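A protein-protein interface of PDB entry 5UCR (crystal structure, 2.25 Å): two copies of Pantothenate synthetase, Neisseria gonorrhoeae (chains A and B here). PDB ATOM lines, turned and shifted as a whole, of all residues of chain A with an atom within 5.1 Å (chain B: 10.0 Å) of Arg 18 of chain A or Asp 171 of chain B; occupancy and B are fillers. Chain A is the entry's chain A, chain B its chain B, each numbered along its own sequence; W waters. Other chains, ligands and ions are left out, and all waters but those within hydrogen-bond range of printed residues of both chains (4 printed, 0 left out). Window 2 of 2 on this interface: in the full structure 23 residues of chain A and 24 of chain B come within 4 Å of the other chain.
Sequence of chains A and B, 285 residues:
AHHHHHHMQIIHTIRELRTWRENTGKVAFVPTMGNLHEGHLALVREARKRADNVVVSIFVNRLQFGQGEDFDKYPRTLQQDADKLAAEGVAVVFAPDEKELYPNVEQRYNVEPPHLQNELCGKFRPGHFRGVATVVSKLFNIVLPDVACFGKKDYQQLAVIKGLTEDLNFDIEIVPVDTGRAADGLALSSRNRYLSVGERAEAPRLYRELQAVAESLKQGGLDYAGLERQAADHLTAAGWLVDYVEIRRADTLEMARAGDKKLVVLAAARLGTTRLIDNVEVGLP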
ATOM      1  N   ILE A  14     -15.084 -25.615  -8.021  1.00  0.00           N
ATOM      2  CA  ILE A  14     -15.365 -24.439  -8.840  1.00  0.00           C
ATOM      3  C   ILE A  14     -16.137 -24.829 -10.093  1.00  0.00           C
ATOM      4  O   ILE A  14     -17.079 -24.132 -10.503  1.00  0.00           O
ATOM      5  CB  ILE A  14     -14.052 -23.716  -9.199  1.00  0.00           C
ATOM      6  CG1 ILE A  14     -13.428 -23.106  -7.945  1.00  0.00           C
ATOM      7  CG2 ILE A  14     -14.294 -22.673 -10.285  1.00  0.00           C
ATOM      8  CD1 ILE A  14     -11.961 -22.773  -8.087  1.00  0.00           C
ATOM      9  N   ARG A  15     -15.744 -25.940 -10.731  1.00  0.00           N
ATOM     10  CA  ARG A  15     -16.358 -26.323 -11.998  1.00  0.00           C
ATOM     11  C   ARG A  15     -17.839 -26.630 -11.821  1.00  0.00           C
ATOM     12  O   ARG A  15     -18.670 -26.238 -12.654  1.00  0.00           O
ATOM     13  CB  ARG A  15     -15.631 -27.529 -12.596  1.00  0.00           C
ATOM     14  N   GLU A  16     -18.191 -27.332 -10.746  1.00  0.00           N
ATOM     15  CA  GLU A  16     -19.599 -27.614 -10.493  1.00  0.00           C
ATOM     16  C   GLU A  16     -20.359 -26.348 -10.109  1.00  0.00           C
ATOM     17  O   GLU A  16     -21.539 -26.214 -10.432  1.00  0.00           O
ATOM     18  CB  GLU A  16     -19.737 -28.661  -9.396  1.00  0.00           C
ATOM     19  CG  GLU A  16     -19.390 -30.068  -9.804  1.00  0.00           C
ATOM     20  CD  GLU A  16     -19.550 -31.020  -8.643  1.00  0.00           C
ATOM     21  OE1 GLU A  16     -18.991 -30.723  -7.559  1.00  0.00           O
ATOM     22  OE2 GLU A  16     -20.258 -32.040  -8.796  1.00  0.00           O
ATOM     23  N   LEU A  17     -19.714 -25.422  -9.396  1.00  0.00           N
ATOM     24  CA  LEU A  17     -20.385 -24.163  -9.075  1.00  0.00           C
ATOM     25  C   LEU A  17     -20.703 -23.389 -10.349  1.00  0.00           C
ATOM     26  O   LEU A  17     -21.828 -22.914 -10.538  1.00  0.00           O
ATOM     27  CB  LEU A  17     -19.522 -23.326  -8.123  1.00  0.00           C
ATOM     28  CG  LEU A  17     -20.199 -22.193  -7.324  1.00  0.00           C
ATOM     29  CD1 LEU A  17     -20.632 -21.007  -8.203  1.00  0.00           C
ATOM     30  CD2 LEU A  17     -21.385 -22.724  -6.527  1.00  0.00           C
ATOM     31  N   ARG A  18     -19.711 -23.262 -11.241  1.00  0.00           N
ATOM     32  CA  ARG A  18     -19.903 -22.549 -12.499  1.00  0.00           C
ATOM     33  C   ARG A  18     -20.985 -23.203 -13.358  1.00  0.00           C
ATOM     34  O   ARG A  18     -21.803 -22.506 -13.971  1.00  0.00           O
ATOM     35  CB  ARG A  18     -18.590 -22.489 -13.275  1.00  0.00           C
ATOM     36  CG  ARG A  18     -17.409 -21.824 -12.564  1.00  0.00           C
ATOM     37  CD  ARG A  18     -16.372 -21.411 -13.609  1.00  0.00           C
ATOM     38  NE  ARG A  18     -15.190 -20.780 -13.031  1.00  0.00           N
ATOM     39  CZ  ARG A  18     -15.116 -19.499 -12.696  1.00  0.00           C
ATOM     40  NH1 ARG A  18     -16.170 -18.702 -12.867  1.00  0.00           N
ATOM     41  NH2 ARG A  18     -13.996 -19.013 -12.175  1.00  0.00           N
ATOM     42  N   THR A  19     -21.000 -24.538 -13.425  1.00  0.00           N
ATOM     43  CA  THR A  19     -22.023 -25.227 -14.213  1.00  0.00           C
ATOM     44  C   THR A  19     -23.423 -24.945 -13.678  1.00  0.00           C
ATOM     45  O   THR A  19     -24.360 -24.716 -14.453  1.00  0.00           O
ATOM     46  CB  THR A  19     -21.771 -26.731 -14.227  1.00  0.00           C
ATOM     47  OG1 THR A  19     -20.515 -27.002 -14.856  1.00  0.00           O
ATOM     48  CG2 THR A  19     -22.885 -27.443 -14.997  1.00  0.00           C
ATOM     49  N   TRP A  20     -23.594 -24.983 -12.357  1.00  0.00           N
ATOM     50  CA  TRP A  20     -24.898 -24.667 -11.785  1.00  0.00           C
ATOM     51  C   TRP A  20     -25.281 -23.215 -12.059  1.00  0.00           C
ATOM     52  O   TRP A  20     -26.435 -22.924 -12.392  1.00  0.00           O
ATOM     53  CB  TRP A  20     -24.896 -24.934 -10.278  1.00  0.00           C
ATOM     54  CG  TRP A  20     -26.069 -24.286  -9.601  1.00  0.00           C
ATOM     55  CD1 TRP A  20     -27.338 -24.803  -9.464  1.00  0.00           C
ATOM     56  CD2 TRP A  20     -26.099 -22.988  -8.999  1.00  0.00           C
ATOM     57  NE1 TRP A  20     -28.141 -23.901  -8.809  1.00  0.00           N
ATOM     58  CE2 TRP A  20     -27.406 -22.780  -8.513  1.00  0.00           C
ATOM     59  CE3 TRP A  20     -25.141 -21.981  -8.814  1.00  0.00           C
ATOM     60  CZ2 TRP A  20     -27.783 -21.610  -7.852  1.00  0.00           C
ATOM     61  CZ3 TRP A  20     -25.523 -20.809  -8.171  1.00  0.00           C
ATOM     62  CH2 TRP A  20     -26.836 -20.640  -7.695  1.00  0.00           C
ATOM     63  N   ARG A  21     -24.319 -22.293 -11.925  1.00  0.00           N
ATOM     64  CA  ARG A  21     -24.605 -20.863 -11.999  1.00  0.00           C
ATOM     65  C   ARG A  21     -24.981 -20.426 -13.405  1.00  0.00           C
ATOM     66  O   ARG A  21     -25.704 -19.437 -13.571  1.00  0.00           O
ATOM     67  CB  ARG A  21     -23.376 -20.078 -11.519  1.00  0.00           C
ATOM     68  CG  ARG A  21     -23.655 -18.647 -11.084  1.00  0.00           C
ATOM     69  CD  ARG A  21     -23.539 -17.669 -12.235  1.00  0.00           C
ATOM     70  NE  ARG A  21     -23.999 -16.335 -11.855  1.00  0.00           N
ATOM     71  CZ  ARG A  21     -25.252 -15.911 -12.027  1.00  0.00           C
ATOM     72  NH1 ARG A  21     -26.164 -16.717 -12.572  1.00  0.00           N
ATOM     73  NH2 ARG A  21     -25.584 -14.674 -11.658  1.00  0.00           N
ATOM     74  N   GLU A  22     -24.495 -21.151 -14.413  1.00  0.00           N
ATOM     75  CA  GLU A  22     -24.633 -20.728 -15.801  1.00  0.00           C
ATOM     76  C   GLU A  22     -26.099 -20.642 -16.218  1.00  0.00           C
ATOM     77  O   GLU A  22     -26.514 -19.680 -16.871  1.00  0.00           O
ATOM     78  CB  GLU A  22     -23.869 -21.704 -16.692  1.00  0.00           C
ATOM     79  CG  GLU A  22     -23.526 -21.200 -18.080  1.00  0.00           C
ATOM     80  CD  GLU A  22     -22.701 -22.212 -18.872  1.00  0.00           C
ATOM     81  OE1 GLU A  22     -22.208 -21.859 -19.966  1.00  0.00           O
ATOM     82  OE2 GLU A  22     -22.542 -23.362 -18.400  1.00  0.00           O
ATOM     83  N   ASN A 141     -15.264 -13.898  -8.652  1.00  0.00           N
ATOM     84  CA  ASN A 141     -14.972 -14.414  -9.985  1.00  0.00           C
ATOM     85  C   ASN A 141     -15.450 -15.839 -10.183  1.00  0.00           C
ATOM     86  O   ASN A 141     -15.598 -16.268 -11.337  1.00  0.00           O
ATOM     87  CB  ASN A 141     -13.467 -14.343 -10.241  1.00  0.00           C
ATOM     88  CG  ASN A 141     -13.052 -13.005 -10.761  1.00  0.00           C
ATOM     89  OD1 ASN A 141     -13.883 -12.274 -11.320  1.00  0.00           O
ATOM     90  ND2 ASN A 141     -11.764 -12.665 -10.608  1.00  0.00           N
ATOM     91  N   ILE A 142     -15.666 -16.590  -9.096  1.00  0.00           N
ATOM     92  CA  ILE A 142     -16.207 -17.941  -9.205  1.00  0.00           C
ATOM     93  C   ILE A 142     -17.733 -17.917  -9.275  1.00  0.00           C
ATOM     94  O   ILE A 142     -18.346 -18.588 -10.112  1.00  0.00           O
ATOM     95  CB  ILE A 142     -15.729 -18.797  -8.016  1.00  0.00           C
ATOM     96  CG1 ILE A 142     -14.203 -18.986  -8.054  1.00  0.00           C
ATOM     97  CG2 ILE A 142     -16.468 -20.125  -7.991  1.00  0.00           C
ATOM     98  CD1 ILE A 142     -13.668 -19.620  -6.804  1.00  0.00           C
ATOM     99  N   LEU A 144     -19.834 -15.223  -9.600  1.00  0.00           N
ATOM    100  CA  LEU A 144     -20.398 -14.212 -10.486  1.00  0.00           C
ATOM    101  C   LEU A 144     -21.770 -13.749  -9.985  1.00  0.00           C
ATOM    102  O   LEU A 144     -22.776 -13.895 -10.687  1.00  0.00           O
ATOM    103  CB  LEU A 144     -20.489 -14.735 -11.914  1.00  0.00           C
ATOM    104  CG  LEU A 144     -19.197 -15.143 -12.649  1.00  0.00           C
ATOM    105  CD1 LEU A 144     -19.525 -15.873 -13.953  1.00  0.00           C
ATOM    106  CD2 LEU A 144     -18.292 -13.943 -12.936  1.00  0.00           C
ATOM    107  N   ARG B  21     -22.923  -6.303 -24.090  1.00  0.00           N
ATOM    108  CA  ARG B  21     -22.315  -7.617 -23.890  1.00  0.00           C
ATOM    109  C   ARG B  21     -23.324  -8.628 -23.356  1.00  0.00           C
ATOM    110  O   ARG B  21     -23.246  -9.816 -23.686  1.00  0.00           O
ATOM    111  CB  ARG B  21     -21.103  -7.491 -22.960  1.00  0.00           C
ATOM    112  CG  ARG B  21     -20.157  -8.687 -22.985  1.00  0.00           C
ATOM    113  CD  ARG B  21     -20.545  -9.786 -21.980  1.00  0.00           C
ATOM    114  NE  ARG B  21     -19.640 -10.935 -22.064  1.00  0.00           N
ATOM    115  CZ  ARG B  21     -19.835 -12.005 -22.831  1.00  0.00           C
ATOM    116  NH1 ARG B  21     -18.937 -12.982 -22.827  1.00  0.00           N
ATOM    117  NH2 ARG B  21     -20.913 -12.108 -23.597  1.00  0.00           N
ATOM    118  N   LYS B  26     -20.333 -15.945 -27.044  1.00  0.00           N
ATOM    119  CA  LYS B  26     -18.905 -16.008 -26.773  1.00  0.00           C
ATOM    120  C   LYS B  26     -18.244 -14.701 -27.189  1.00  0.00           C
ATOM    121  O   LYS B  26     -18.529 -14.159 -28.258  1.00  0.00           O
ATOM    122  CB  LYS B  26     -18.290 -17.190 -27.531  1.00  0.00           C
ATOM    123  CG  LYS B  26     -17.003 -17.761 -26.946  1.00  0.00           C
ATOM    124  CD  LYS B  26     -16.651 -19.087 -27.630  1.00  0.00           C
ATOM    125  CE  LYS B  26     -15.488 -19.808 -26.952  1.00  0.00           C
ATOM    126  NZ  LYS B  26     -14.224 -19.820 -27.760  1.00  0.00           N
ATOM    127  N   VAL B  27     -17.368 -14.181 -26.336  1.00  0.00           N
ATOM    128  CA  VAL B  27     -16.647 -12.946 -26.621  1.00  0.00           C
ATOM    129  C   VAL B  27     -15.152 -13.206 -26.488  1.00  0.00           C
ATOM    130  O   VAL B  27     -14.698 -13.733 -25.468  1.00  0.00           O
ATOM    131  CB  VAL B  27     -17.079 -11.793 -25.696  1.00  0.00           C
ATOM    132  CG1 VAL B  27     -16.068 -10.662 -25.780  1.00  0.00           C
ATOM    133  CG2 VAL B  27     -18.482 -11.282 -26.084  1.00  0.00           C
ATOM    134  N   PHE B 140     -11.134  -7.003 -17.654  1.00  0.00           N
ATOM    135  CA  PHE B 140     -11.750  -8.323 -17.556  1.00  0.00           C
ATOM    136  C   PHE B 140     -13.123  -8.252 -16.881  1.00  0.00           C
ATOM    137  O   PHE B 140     -14.072  -8.902 -17.324  1.00  0.00           O
ATOM    138  CB  PHE B 140     -10.842  -9.275 -16.774  1.00  0.00           C
ATOM    139  CG  PHE B 140      -9.716  -9.909 -17.591  1.00  0.00           C
ATOM    140  CD1 PHE B 140      -9.623  -9.732 -18.955  1.00  0.00           C
ATOM    141  CD2 PHE B 140      -8.768 -10.705 -16.958  1.00  0.00           C
ATOM    142  CE1 PHE B 140      -8.600 -10.319 -19.676  1.00  0.00           C
ATOM    143  CE2 PHE B 140      -7.743 -11.297 -17.672  1.00  0.00           C
ATOM    144  CZ  PHE B 140      -7.656 -11.106 -19.029  1.00  0.00           C
ATOM    145  N   ASN B 141     -13.235  -7.503 -15.779  1.00  0.00           N
ATOM    146  CA  ASN B 141     -14.509  -7.401 -15.090  1.00  0.00           C
ATOM    147  C   ASN B 141     -15.500  -6.530 -15.832  1.00  0.00           C
ATOM    148  O   ASN B 141     -16.696  -6.610 -15.540  1.00  0.00           O
ATOM    149  CB  ASN B 141     -14.331  -6.839 -13.680  1.00  0.00           C
ATOM    150  CG  ASN B 141     -13.851  -7.870 -12.706  1.00  0.00           C
ATOM    151  OD1 ASN B 141     -14.063  -9.063 -12.916  1.00  0.00           O
ATOM    152  ND2 ASN B 141     -13.197  -7.423 -11.622  1.00  0.00           N
ATOM    153  N   VAL B 143     -15.533  -6.338 -19.477  1.00  0.00           N
ATOM    154  CA  VAL B 143     -15.906  -6.995 -20.728  1.00  0.00           C
ATOM    155  C   VAL B 143     -16.479  -8.389 -20.487  1.00  0.00           C
ATOM    156  O   VAL B 143     -17.278  -8.874 -21.290  1.00  0.00           O
ATOM    157  CB  VAL B 143     -14.698  -7.051 -21.687  1.00  0.00           C
ATOM    158  CG1 VAL B 143     -14.995  -7.913 -22.895  1.00  0.00           C
ATOM    159  CG2 VAL B 143     -14.289  -5.650 -22.163  1.00  0.00           C
ATOM    160  N   LEU B 144     -16.110  -9.028 -19.386  1.00  0.00           N
ATOM    161  CA  LEU B 144     -16.481 -10.411 -19.104  1.00  0.00           C
ATOM    162  C   LEU B 144     -16.239 -11.308 -20.316  1.00  0.00           C
ATOM    163  O   LEU B 144     -17.185 -11.945 -20.821  1.00  0.00           O
ATOM    164  CB  LEU B 144     -17.932 -10.491 -18.647  1.00  0.00           C
ATOM    165  CG  LEU B 144     -18.268  -9.650 -17.410  1.00  0.00           C
ATOM    166  CD1 LEU B 144     -19.741  -9.728 -17.042  1.00  0.00           C
ATOM    167  CD2 LEU B 144     -17.373 -10.076 -16.230  1.00  0.00           C
ATOM    168  N   PRO B 145     -15.009 -11.396 -20.820  1.00  0.00           N
ATOM    169  CA  PRO B 145     -14.753 -12.181 -22.029  1.00  0.00           C
ATOM    170  C   PRO B 145     -14.661 -13.664 -21.699  1.00  0.00           C
ATOM    171  O   PRO B 145     -14.513 -14.073 -20.547  1.00  0.00           O
ATOM    172  CB  PRO B 145     -13.407 -11.640 -22.510  1.00  0.00           C
ATOM    173  CG  PRO B 145     -12.686 -11.403 -21.247  1.00  0.00           C
ATOM    174  CD  PRO B 145     -13.751 -10.826 -20.294  1.00  0.00           C
ATOM    175  N   ASP B 146     -14.775 -14.472 -22.746  1.00  0.00           N
ATOM    176  CA  ASP B 146     -14.491 -15.897 -22.659  1.00  0.00           C
ATOM    177  C   ASP B 146     -13.065 -16.234 -23.086  1.00  0.00           C
ATOM    178  O   ASP B 146     -12.482 -17.187 -22.564  1.00  0.00           O
ATOM    179  CB  ASP B 146     -15.495 -16.671 -23.520  1.00  0.00           C
ATOM    180  CG  ASP B 146     -16.929 -16.445 -23.073  1.00  0.00           C
ATOM    181  OD1 ASP B 146     -17.298 -16.934 -21.984  1.00  0.00           O
ATOM    182  OD2 ASP B 146     -17.675 -15.740 -23.771  1.00  0.00           O
ATOM    183  N   VAL B 147     -12.489 -15.450 -23.997  1.00  0.00           N
ATOM    184  CA  VAL B 147     -11.122 -15.634 -24.473  1.00  0.00           C
ATOM    185  C   VAL B 147     -10.442 -14.268 -24.551  1.00  0.00           C
ATOM    186  O   VAL B 147     -11.070 -13.265 -24.905  1.00  0.00           O
ATOM    187  CB  VAL B 147     -11.103 -16.352 -25.852  1.00  0.00           C
ATOM    188  CG1 VAL B 147      -9.679 -16.610 -26.318  1.00  0.00           C
ATOM    189  CG2 VAL B 147     -11.882 -17.657 -25.800  1.00  0.00           C
ATOM    190  N   ALA B 148      -9.147 -14.226 -24.226  1.00  0.00           N
ATOM    191  CA  ALA B 148      -8.378 -12.982 -24.313  1.00  0.00           C
ATOM    192  C   ALA B 148      -7.020 -13.266 -24.933  1.00  0.00           C
ATOM    193  O   ALA B 148      -6.337 -14.206 -24.512  1.00  0.00           O
ATOM    194  CB  ALA B 148      -8.204 -12.323 -22.932  1.00  0.00           C
ATOM    195  N   ILE B 161      -0.325 -11.851 -16.764  1.00  0.00           N
ATOM    196  CA  ILE B 161      -1.753 -11.998 -17.031  1.00  0.00           C
ATOM    197  C   ILE B 161      -2.204 -13.442 -16.822  1.00  0.00           C
ATOM    198  O   ILE B 161      -3.253 -13.689 -16.215  1.00  0.00           O
ATOM    199  CB  ILE B 161      -2.073 -11.489 -18.447  1.00  0.00           C
ATOM    200  CG1 ILE B 161      -1.905  -9.968 -18.466  1.00  0.00           C
ATOM    201  CG2 ILE B 161      -3.519 -11.870 -18.852  1.00  0.00           C
ATOM    202  CD1 ILE B 161      -1.674  -9.382 -19.827  1.00  0.00           C
ATOM    203  N   LYS B 162      -1.430 -14.425 -17.316  1.00  0.00           N
ATOM    204  CA  LYS B 162      -1.761 -15.817 -17.017  1.00  0.00           C
ATOM    205  C   LYS B 162      -1.804 -16.047 -15.507  1.00  0.00           C
ATOM    206  O   LYS B 162      -2.729 -16.697 -14.995  1.00  0.00           O
ATOM    207  CB  LYS B 162      -0.762 -16.771 -17.698  1.00  0.00           C
ATOM    208  N   LEU B 164      -2.358 -13.841 -12.947  1.00  0.00           N
ATOM    209  CA  LEU B 164      -3.500 -13.237 -12.262  1.00  0.00           C
ATOM    210  C   LEU B 164      -4.792 -13.973 -12.614  1.00  0.00           C
ATOM    211  O   LEU B 164      -5.647 -14.190 -11.749  1.00  0.00           O
ATOM    212  CB  LEU B 164      -3.589 -11.742 -12.590  1.00  0.00           C
ATOM    213  CG  LEU B 164      -4.096 -11.226 -13.939  1.00  0.00           C
ATOM    214  CD1 LEU B 164      -5.600 -11.120 -13.965  1.00  0.00           C
ATOM    215  CD2 LEU B 164      -3.462  -9.855 -14.233  1.00  0.00           C
ATOM    216  N   THR B 165      -4.929 -14.392 -13.875  1.00  0.00           N
ATOM    217  CA  THR B 165      -6.099 -15.152 -14.292  1.00  0.00           C
ATOM    218  C   THR B 165      -6.270 -16.410 -13.435  1.00  0.00           C
ATOM    219  O   THR B 165      -7.361 -16.665 -12.901  1.00  0.00           O
ATOM    220  CB  THR B 165      -5.985 -15.496 -15.781  1.00  0.00           C
ATOM    221  OG1 THR B 165      -5.860 -14.288 -16.560  1.00  0.00           O
ATOM    222  CG2 THR B 165      -7.224 -16.268 -16.254  1.00  0.00           C
ATOM    223  N   GLU B 166      -5.197 -17.198 -13.272  1.00  0.00           N
ATOM    224  CA  GLU B 166      -5.260 -18.381 -12.412  1.00  0.00           C
ATOM    225  C   GLU B 166      -5.545 -18.011 -10.959  1.00  0.00           C
ATOM    226  O   GLU B 166      -6.437 -18.584 -10.322  1.00  0.00           O
ATOM    227  CB  GLU B 166      -3.951 -19.164 -12.477  1.00  0.00           C
ATOM    228  CG  GLU B 166      -3.711 -19.975 -13.726  1.00  0.00           C
ATOM    229  CD  GLU B 166      -2.265 -20.455 -13.817  1.00  0.00           C
ATOM    230  OE1 GLU B 166      -1.611 -20.589 -12.755  1.00  0.00           O
ATOM    231  OE2 GLU B 166      -1.783 -20.677 -14.950  1.00  0.00           O
ATOM    232  N   ASP B 167      -4.763 -17.086 -10.399  1.00  0.00           N
ATOM    233  CA  ASP B 167      -4.805 -16.839  -8.959  1.00  0.00           C
ATOM    234  C   ASP B 167      -6.081 -16.142  -8.525  1.00  0.00           C
ATOM    235  O   ASP B 167      -6.447 -16.226  -7.349  1.00  0.00           O
ATOM    236  CB  ASP B 167      -3.623 -15.978  -8.512  1.00  0.00           C
ATOM    237  CG  ASP B 167      -2.382 -16.790  -8.189  1.00  0.00           C
ATOM    238  OD1 ASP B 167      -2.329 -18.002  -8.512  1.00  0.00           O
ATOM    239  OD2 ASP B 167      -1.448 -16.205  -7.601  1.00  0.00           O
ATOM    240  N   LEU B 168      -6.747 -15.441  -9.437  1.00  0.00           N
ATOM    241  CA  LEU B 168      -7.985 -14.743  -9.122  1.00  0.00           C
ATOM    242  C   LEU B 168      -9.215 -15.432  -9.693  1.00  0.00           C
ATOM    243  O   LEU B 168     -10.316 -14.901  -9.546  1.00  0.00           O
ATOM    244  CB  LEU B 168      -7.912 -13.290  -9.621  1.00  0.00           C
ATOM    245  CG  LEU B 168      -6.770 -12.485  -8.979  1.00  0.00           C
ATOM    246  CD1 LEU B 168      -6.694 -11.060  -9.543  1.00  0.00           C
ATOM    247  CD2 LEU B 168      -6.916 -12.475  -7.445  1.00  0.00           C
ATOM    248  N   ASN B 169      -9.055 -16.585 -10.353  1.00  0.00           N
ATOM    249  CA  ASN B 169     -10.182 -17.406 -10.828  1.00  0.00           C
ATOM    250  C   ASN B 169     -11.024 -16.691 -11.889  1.00  0.00           C
ATOM    251  O   ASN B 169     -12.248 -16.859 -11.959  1.00  0.00           O
ATOM    252  CB  ASN B 169     -11.058 -17.866  -9.654  1.00  0.00           C
ATOM    253  CG  ASN B 169     -10.288 -18.695  -8.644  1.00  0.00           C
ATOM    254  OD1 ASN B 169      -9.938 -18.205  -7.566  1.00  0.00           O
ATOM    255  ND2 ASN B 169      -9.997 -19.959  -9.000  1.00  0.00           N
ATOM    256  N   PHE B 170     -10.370 -15.891 -12.730  1.00  0.00           N
ATOM    257  CA  PHE B 170     -11.032 -15.361 -13.914  1.00  0.00           C
ATOM    258  C   PHE B 170     -11.312 -16.511 -14.866  1.00  0.00           C
ATOM    259  O   PHE B 170     -10.384 -17.206 -15.291  1.00  0.00           O
ATOM    260  CB  PHE B 170     -10.170 -14.309 -14.610  1.00  0.00           C
ATOM    261  CG  PHE B 170     -10.269 -12.923 -14.009  1.00  0.00           C
ATOM    262  CD1 PHE B 170     -11.406 -12.127 -14.226  1.00  0.00           C
ATOM    263  CD2 PHE B 170      -9.208 -12.396 -13.269  1.00  0.00           C
ATOM    264  CE1 PHE B 170     -11.482 -10.833 -13.693  1.00  0.00           C
ATOM    265  CE2 PHE B 170      -9.274 -11.108 -12.725  1.00  0.00           C
ATOM    266  CZ  PHE B 170     -10.419 -10.324 -12.935  1.00  0.00           C
ATOM    267  N   ASP B 171     -12.586 -16.708 -15.213  1.00  0.00           N
ATOM    268  CA  ASP B 171     -12.968 -17.783 -16.124  1.00  0.00           C
ATOM    269  C   ASP B 171     -12.727 -17.335 -17.564  1.00  0.00           C
ATOM    270  O   ASP B 171     -13.646 -17.103 -18.343  1.00  0.00           O
ATOM    271  CB  ASP B 171     -14.420 -18.179 -15.910  1.00  0.00           C
ATOM    272  CG  ASP B 171     -14.779 -19.450 -16.646  1.00  0.00           C
ATOM    273  OD1 ASP B 171     -13.852 -20.200 -16.988  1.00  0.00           O
ATOM    274  OD2 ASP B 171     -15.980 -19.703 -16.879  1.00  0.00           O
ATOM    275  N   ILE B 172     -11.448 -17.205 -17.916  1.00  0.00           N
ATOM    276  CA  ILE B 172     -11.059 -16.621 -19.196  1.00  0.00           C
ATOM    277  C   ILE B 172      -9.914 -17.434 -19.777  1.00  0.00           C
ATOM    278  O   ILE B 172      -8.895 -17.653 -19.110  1.00  0.00           O
ATOM    279  CB  ILE B 172     -10.628 -15.146 -19.070  1.00  0.00           C
ATOM    280  CG1 ILE B 172     -11.697 -14.303 -18.381  1.00  0.00           C
ATOM    281  CG2 ILE B 172     -10.359 -14.577 -20.440  1.00  0.00           C
ATOM    282  CD1 ILE B 172     -11.295 -12.848 -18.190  1.00  0.00           C
ATOM    283  N   GLU B 173     -10.060 -17.846 -21.029  1.00  0.00           N
ATOM    284  CA  GLU B 173      -8.978 -18.542 -21.713  1.00  0.00           C
ATOM    285  C   GLU B 173      -7.973 -17.519 -22.242  1.00  0.00           C
ATOM    286  O   GLU B 173      -8.319 -16.657 -23.059  1.00  0.00           O
ATOM    287  CB  GLU B 173      -9.536 -19.411 -22.837  1.00  0.00           C
ATOM    288  CG  GLU B 173      -8.496 -20.302 -23.502  1.00  0.00           C
ATOM    289  CD  GLU B 173      -9.064 -21.067 -24.676  1.00  0.00           C
ATOM    290  OE1 GLU B 173      -8.262 -21.657 -25.433  1.00  0.00           O
ATOM    291  OE2 GLU B 173     -10.311 -21.072 -24.840  1.00  0.00           O
ATOM    292  N   ILE B 174      -6.740 -17.604 -21.759  1.00  0.00           N
ATOM    293  CA  ILE B 174      -5.660 -16.727 -22.199  1.00  0.00           C
ATOM    294  C   ILE B 174      -4.962 -17.386 -23.382  1.00  0.00           C
ATOM    295  O   ILE B 174      -4.420 -18.487 -23.251  1.00  0.00           O
ATOM    296  CB  ILE B 174      -4.667 -16.460 -21.057  1.00  0.00           C
ATOM    297  CG1 ILE B 174      -5.397 -15.888 -19.833  1.00  0.00           C
ATOM    298  CG2 ILE B 174      -3.580 -15.531 -21.514  1.00  0.00           C
ATOM    299  CD1 ILE B 174      -6.316 -14.684 -20.149  1.00  0.00           C
HETATM  300  O   HOH W   1     -16.471 -10.404 -12.499  1.00  0.00           O
HETATM  301  O   HOH W   2     -15.174 -12.272 -13.628  1.00  0.00           O
HETATM  302  O   HOH W   3     -14.879 -15.056 -13.640  1.00  0.00           O
HETATM  303  O   HOH W   4     -11.354 -20.751 -11.934  1.00  0.00           O
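O of Asn 169 of chain B is in hydrogen-bond range of NH2 of Arg 18 of chain A. ND2 of Asn 141 of chain A sits at hydrogen-bond distance from O of Leu 168 of chain B, at 2.9 Å. O of Asn 141 of chain A lies close to O of Asn 169 of chain B, 3.5 Å away.
The guanidinium group of Arg 18 of chain A lies within hydrogen-bond range of the backbone carbonyl oxygen of Asn 141 of chain A (2.9 Å). The backbone carbonyl oxygen (O) of Thr 165 of chain B sits at hydrogen-bond distance from the backbone NH (N) of Phe 170 of chain B.
CD1 of Ile 14 of chain A touches ND2 of Asn 169 of chain B (3.6 Å). CZ of Arg 18 of chain A touches CB of Asp 171 of chain B, 3.5 Å away. OD1 of Asn 141 of chain A touches OD1 of Asn 141 of chain B, 3.6 Å away. Phe 170 of chain B touches Asn 141 of chain A (CZ to ND2, 3.6 Å). CG1 of Ile 142 of chain A touches CB of Asn 169 of chain B (3.7 Å).
Of the printed residues of chain B, Ile 14 of chain A touches Asn 169 (3.6 Å). No residue of chain B comes within 4 Å of Arg 15 of chain A. No residue of chain B comes within 4 Å of Leu 17 of chain A. Ile 142 of chain A touches one residue of chain B. Of the printed residues of chain A, Asn 141 of chain B touches Asn 141. Glu 166 of chain B touches none of the printed residues of chain A. Printed residues of chain A within 4 Å of Phe 170 of chain B: Asn 141 (3.6 Å). Of chain A, only Arg 18 (3.5 Å) comes within 4 Å of Asp 171 of chain B. Ile 172 of chain B touches none of the printed residues of chain A. The nearest residue of chain B that does not touch Arg 18 of chain A is Phe 170 of chain B (4.6 Å). The nearest printed residue of chain A that does not touch Leu 168 of chain B is Ile 142 of chain A (5.6 Å).
Printed residues of chain A that touch a printed residue of chain B: Ile 14, Arg 18, Asn 141 and Ile 142. Printed residues of chain B that touch a printed residue of chain A: Asn 141, Leu 168, Asn 169, Phe 170 and Asp 171. Hydrophobic or aromatic side chains of chain B within 4 Å of the printed part of chain A: Phe 170.
Asn 141 of chain A touches its own counterpart, Asn 141 of chain B.
Water W2 bridges OD1 of Asn 141 of chain A (2.6 Å) and OD1 of Asn 141 of chain B (3.5 Å). Water W3 lies within hydrogen-bond range of O of Asn 141 of chain A and N of Asp 171 of chain B. Water W1 lies within hydrogen-bond range of the side-chain amide oxygen (OD1) of Asn 141 of chain B (2.8 Å) and the side-chain amide oxygen (OD1) of Asn 141 of chain A (3.4 Å). Water W4 bridges the guanidinium group (NH2) of Arg 18 of chain A and the side-chain amide nitrogen (ND2) of Asn 169 of chain B.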
